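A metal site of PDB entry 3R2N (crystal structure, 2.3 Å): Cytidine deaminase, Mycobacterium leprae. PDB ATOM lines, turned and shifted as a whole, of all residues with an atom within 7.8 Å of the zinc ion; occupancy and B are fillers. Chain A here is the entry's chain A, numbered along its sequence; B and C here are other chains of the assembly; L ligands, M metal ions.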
ATOM      1  N   ALA A  58       4.444  -5.703  38.062  1.00  0.00           N
ATOM      2  CA  ALA A  58       4.120  -5.160  36.743  1.00  0.00           C
ATOM      3  C   ALA A  58       4.251  -6.183  35.634  1.00  0.00           C
ATOM      4  O   ALA A  58       5.240  -6.903  35.562  1.00  0.00           O
ATOM      5  CB  ALA A  58       5.028  -3.945  36.401  1.00  0.00           C
ATOM      6  N   LEU A  59       3.261  -6.235  34.748  1.00  0.00           N
ATOM      7  CA  LEU A  59       3.355  -7.067  33.519  1.00  0.00           C
ATOM      8  C   LEU A  59       3.751  -6.161  32.363  1.00  0.00           C
ATOM      9  O   LEU A  59       3.170  -5.097  32.170  1.00  0.00           O
ATOM     10  CB  LEU A  59       2.023  -7.753  33.225  1.00  0.00           C
ATOM     11  CG  LEU A  59       1.501  -8.715  34.276  1.00  0.00           C
ATOM     12  CD1 LEU A  59      -0.034  -8.960  34.184  1.00  0.00           C
ATOM     13  CD2 LEU A  59       2.274 -10.019  34.123  1.00  0.00           C
ATOM     14  N   CYS A  60       4.760  -6.584  31.599  1.00  0.00           N
ATOM     15  CA  CYS A  60       5.207  -5.852  30.423  1.00  0.00           C
ATOM     16  C   CYS A  60       4.187  -6.053  29.292  1.00  0.00           C
ATOM     17  O   CYS A  60       3.433  -7.064  29.296  1.00  0.00           O
ATOM     18  CB  CYS A  60       6.593  -6.349  29.986  1.00  0.00           C
ATOM     19  SG  CYS A  60       8.037  -5.545  30.810  1.00  0.00           S
ATOM     20  N   ALA A  61       4.189  -5.125  28.317  1.00  0.00           N
ATOM     21  CA  ALA A  61       3.389  -5.322  27.079  1.00  0.00           C
ATOM     22  C   ALA A  61       3.608  -6.696  26.432  1.00  0.00           C
ATOM     23  O   ALA A  61       2.637  -7.413  26.108  1.00  0.00           O
ATOM     24  CB  ALA A  61       3.623  -4.223  26.104  1.00  0.00           C
ATOM     25  N   GLU A  62       4.860  -7.065  26.251  1.00  0.00           N
ATOM     26  CA  GLU A  62       5.226  -8.348  25.706  1.00  0.00           C
ATOM     27  C   GLU A  62       4.654  -9.506  26.524  1.00  0.00           C
ATOM     28  O   GLU A  62       4.317 -10.554  25.957  1.00  0.00           O
ATOM     29  CB  GLU A  62       6.736  -8.511  25.602  1.00  0.00           C
ATOM     30  CG  GLU A  62       7.442  -7.483  24.742  1.00  0.00           C
ATOM     31  CD  GLU A  62       7.902  -6.287  25.543  1.00  0.00           C
ATOM     32  OE1 GLU A  62       7.063  -5.593  26.177  1.00  0.00           O
ATOM     33  OE2 GLU A  62       9.116  -5.994  25.510  1.00  0.00           O
ATOM     34  N   CYS A  63       4.556  -9.361  27.843  1.00  0.00           N
ATOM     35  CA  CYS A  63       3.997 -10.443  28.676  1.00  0.00           C
ATOM     36  C   CYS A  63       2.539 -10.596  28.350  1.00  0.00           C
ATOM     37  O   CYS A  63       2.030 -11.725  28.339  1.00  0.00           O
ATOM     38  CB  CYS A  63       4.112 -10.201  30.189  1.00  0.00           C
ATOM     39  SG  CYS A  63       5.757  -9.921  30.911  1.00  0.00           S
ATOM     40  N   CYS A  82       7.286  -3.381  19.337  1.00  0.00           N
ATOM     41  CA  CYS A  82       6.958  -2.679  20.561  1.00  0.00           C
ATOM     42  C   CYS A  82       7.107  -1.171  20.368  1.00  0.00           C
ATOM     43  O   CYS A  82       8.093  -0.694  19.766  1.00  0.00           O
ATOM     44  CB  CYS A  82       7.882  -3.171  21.668  1.00  0.00           C
ATOM     45  SG  CYS A  82       7.410  -2.689  23.326  1.00  0.00           S
ATOM     46  N   MET A  91      12.910  -1.172  22.663  1.00  0.00           N
ATOM     47  CA  MET A  91      13.598  -2.455  22.842  1.00  0.00           C
ATOM     48  C   MET A  91      12.967  -3.296  23.966  1.00  0.00           C
ATOM     49  O   MET A  91      12.637  -2.780  25.023  1.00  0.00           O
ATOM     50  CB  MET A  91      15.053  -2.194  23.191  1.00  0.00           C
ATOM     51  CG  MET A  91      15.919  -1.866  21.998  1.00  0.00           C
ATOM     52  SD  MET A  91      15.969  -3.237  20.798  1.00  0.00           S
ATOM     53  CE  MET A  91      16.560  -4.614  21.773  1.00  0.00           C
ATOM     54  N   PRO A  92      12.762  -4.604  23.732  1.00  0.00           N
ATOM     55  CA  PRO A  92      12.274  -5.328  24.911  1.00  0.00           C
ATOM     56  C   PRO A  92      13.299  -5.441  26.054  1.00  0.00           C
ATOM     57  O   PRO A  92      14.492  -5.590  25.815  1.00  0.00           O
ATOM     58  CB  PRO A  92      11.926  -6.707  24.349  1.00  0.00           C
ATOM     59  CG  PRO A  92      11.574  -6.441  22.921  1.00  0.00           C
ATOM     60  CD  PRO A  92      12.537  -5.350  22.484  1.00  0.00           C
ATOM     61  N   CYS A  93      12.828  -5.340  27.284  1.00  0.00           N
ATOM     62  CA  CYS A  93      13.686  -5.558  28.459  1.00  0.00           C
ATOM     63  C   CYS A  93      14.186  -7.010  28.418  1.00  0.00           C
ATOM     64  O   CYS A  93      13.590  -7.873  27.758  1.00  0.00           O
ATOM     65  CB  CYS A  93      12.941  -5.252  29.759  1.00  0.00           C
ATOM     66  SG  CYS A  93      11.802  -6.570  30.395  1.00  0.00           S
ATOM     67  N   GLY A  94      15.298  -7.270  29.114  1.00  0.00           N
ATOM     68  CA  GLY A  94      15.867  -8.601  29.118  1.00  0.00           C
ATOM     69  C   GLY A  94      14.869  -9.690  29.446  1.00  0.00           C
ATOM     70  O   GLY A  94      14.905 -10.744  28.835  1.00  0.00           O
ATOM     71  N   ARG A  95      13.975  -9.481  30.408  1.00  0.00           N
ATOM     72  CA  ARG A  95      12.993 -10.536  30.756  1.00  0.00           C
ATOM     73  C   ARG A  95      12.076 -10.847  29.568  1.00  0.00           C
ATOM     74  O   ARG A  95      11.716 -11.997  29.332  1.00  0.00           O
ATOM     75  CB  ARG A  95      12.175 -10.106  31.970  1.00  0.00           C
ATOM     76  CG  ARG A  95      11.066 -11.065  32.429  1.00  0.00           C
ATOM     77  CD  ARG A  95       9.686 -10.738  31.777  1.00  0.00           C
ATOM     78  NE  ARG A  95       9.219  -9.361  31.983  1.00  0.00           N
ATOM     79  CZ  ARG A  95       8.531  -8.955  33.060  1.00  0.00           C
ATOM     80  NH1 ARG A  95       8.235  -9.806  34.047  1.00  0.00           N
ATOM     81  NH2 ARG A  95       8.145  -7.692  33.147  1.00  0.00           N
ATOM     82  N   CYS A  96      11.721  -9.827  28.791  1.00  0.00           N
ATOM     83  CA  CYS A  96      10.802 -10.026  27.676  1.00  0.00           C
ATOM     84  C   CYS A  96      11.467 -10.737  26.500  1.00  0.00           C
ATOM     85  O   CYS A  96      10.805 -11.497  25.747  1.00  0.00           O
ATOM     86  CB  CYS A  96      10.058  -8.729  27.303  1.00  0.00           C
ATOM     87  SG  CYS A  96       8.892  -8.181  28.620  1.00  0.00           S
ATOM     88  N   ARG A  97      12.782 -10.531  26.392  1.00  0.00           N
ATOM     89  CA  ARG A  97      13.635 -11.227  25.420  1.00  0.00           C
ATOM     90  C   ARG A  97      13.638 -12.717  25.679  1.00  0.00           C
ATOM     91  O   ARG A  97      13.631 -13.507  24.732  1.00  0.00           O
ATOM     92  CB  ARG A  97      15.082 -10.703  25.475  1.00  0.00           C
ATOM     93  CG  ARG A  97      15.194  -9.342  24.846  1.00  0.00           C
ATOM     94  CD  ARG A  97      16.618  -8.842  24.711  1.00  0.00           C
ATOM     95  NE  ARG A  97      16.665  -7.392  24.821  1.00  0.00           N
ATOM     96  CZ  ARG A  97      17.703  -6.622  24.460  1.00  0.00           C
ATOM     97  NH1 ARG A  97      18.784  -7.127  23.895  1.00  0.00           N
ATOM     98  NH2 ARG A  97      17.631  -5.320  24.669  1.00  0.00           N
ATOM     99  N   LEU A  99      11.161 -14.297  27.238  1.00  0.00           N
ATOM    100  CA  LEU A  99       9.798 -14.739  26.867  1.00  0.00           C
ATOM    101  C   LEU A  99       9.688 -14.860  25.359  1.00  0.00           C
ATOM    102  O   LEU A  99       9.166 -15.836  24.856  1.00  0.00           O
ATOM    103  CB  LEU A  99       8.687 -13.820  27.412  1.00  0.00           C
ATOM    104  CG  LEU A  99       8.385 -13.600  28.904  1.00  0.00           C
ATOM    105  CD1 LEU A  99       6.940 -13.033  29.103  1.00  0.00           C
ATOM    106  CD2 LEU A  99       8.500 -14.809  29.796  1.00  0.00           C
ATOM    107  N   SER B  54      13.094  -1.615  34.157  1.00  0.00           N
ATOM    108  CA  SER B  54      11.883  -2.408  33.851  1.00  0.00           C
ATOM    109  C   SER B  54      11.194  -2.785  35.171  1.00  0.00           C
ATOM    110  O   SER B  54      11.742  -3.546  35.984  1.00  0.00           O
ATOM    111  CB  SER B  54      12.254  -3.654  33.055  1.00  0.00           C
ATOM    112  OG  SER B  54      11.099  -4.409  32.758  1.00  0.00           O
ATOM    113  N   TYR B  55      10.008  -2.223  35.395  1.00  0.00           N
ATOM    114  CA  TYR B  55       9.449  -2.208  36.743  1.00  0.00           C
ATOM    115  C   TYR B  55       9.257  -3.591  37.353  1.00  0.00           C
ATOM    116  O   TYR B  55       9.599  -3.793  38.530  1.00  0.00           O
ATOM    117  CB  TYR B  55       8.184  -1.334  36.857  1.00  0.00           C
ATOM    118  CG  TYR B  55       8.447   0.169  36.943  1.00  0.00           C
ATOM    119  CD1 TYR B  55       9.650   0.703  36.473  1.00  0.00           C
ATOM    120  CD2 TYR B  55       7.480   1.054  37.431  1.00  0.00           C
ATOM    121  CE1 TYR B  55       9.896   2.055  36.519  1.00  0.00           C
ATOM    122  CE2 TYR B  55       7.722   2.423  37.476  1.00  0.00           C
ATOM    123  CZ  TYR B  55       8.943   2.914  37.006  1.00  0.00           C
ATOM    124  OH  TYR B  55       9.247   4.273  37.020  1.00  0.00           O
ATOM    125  N   GLY B  56       8.814  -4.540  36.520  1.00  0.00           N
ATOM    126  CA  GLY B  56       8.558  -5.955  36.901  1.00  0.00           C
ATOM    127  C   GLY B  56       9.775  -6.806  37.279  1.00  0.00           C
ATOM    128  O   GLY B  56       9.660  -7.996  37.633  1.00  0.00           O
ATOM    129  N   LEU B  57      10.960  -6.212  37.220  1.00  0.00           N
ATOM    130  CA  LEU B  57      12.136  -6.953  37.616  1.00  0.00           C
ATOM    131  C   LEU B  57      12.689  -6.453  38.955  1.00  0.00           C
ATOM    132  O   LEU B  57      13.799  -6.846  39.366  1.00  0.00           O
ATOM    133  CB  LEU B  57      13.178  -6.916  36.482  1.00  0.00           C
ATOM    134  CG  LEU B  57      12.670  -7.237  35.069  1.00  0.00           C
ATOM    135  CD1 LEU B  57      13.806  -7.216  34.066  1.00  0.00           C
ATOM    136  CD2 LEU B  57      11.903  -8.550  34.963  1.00  0.00           C
ATOM    137  N   GLN C  98      19.198  -8.118  32.364  1.00  0.00           N
ATOM    138  CA  GLN C  98      18.747  -6.764  32.686  1.00  0.00           C
ATOM    139  C   GLN C  98      19.201  -6.309  34.081  1.00  0.00           C
ATOM    140  O   GLN C  98      19.657  -5.166  34.230  1.00  0.00           O
ATOM    141  CB  GLN C  98      17.228  -6.640  32.523  1.00  0.00           C
ATOM    142  CG  GLN C  98      16.672  -5.201  32.404  1.00  0.00           C
ATOM    143  CD  GLN C  98      17.061  -4.533  31.105  1.00  0.00           C
ATOM    144  OE1 GLN C  98      16.800  -5.062  30.022  1.00  0.00           O
ATOM    145  NE2 GLN C  98      17.653  -3.336  31.195  1.00  0.00           N
HETATM  146  C1  LIG L   1       9.066  -2.766  26.814  1.00  0.00           C
HETATM  147  O1  LIG L   1       7.810  -3.322  27.251  1.00  0.00           O
HETATM  148  C2  LIG L   1      10.126  -3.140  27.851  1.00  0.00           C
HETATM  149  O2  LIG L   1      10.340  -4.546  27.795  1.00  0.00           O
HETATM  150 ZN    ZN M   1       9.829  -6.285  29.382  1.00  0.00          ZN
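The side-chain sulfur (SG) of Cys 93 lies close to the backbone NH (N) of Arg 95 (3.6 Å). SG of Cys 93 sits close to OG of Ser 54 of chain B, at 3.3 Å. The side-chain sulfur (SG) of Cys 63 sits at hydrogen-bond distance from the backbone NH (N) of Cys 60 (3.6 Å). The guanidinium group of Arg 95 sits close to the side-chain sulfur of Cys 60 (3.2 Å). SG of Cys 96 sits close to NE of Arg 95 (3.6 Å).
Merely in contact with the zinc ion: Glu 62. Of the 20 residues printed, 4 come within 4 Å of the zinc ion. The nearest printed residue that does not touch the zinc ion is Ser 54 of chain B (4.1 Å).
The zinc ion is bound by SG of Cys 93 (2.2 Å), SG of Cys 96 (2.2 Å), SG of Cys 60 (2.4 Å) and O2 of the ligand (2.4 Å).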
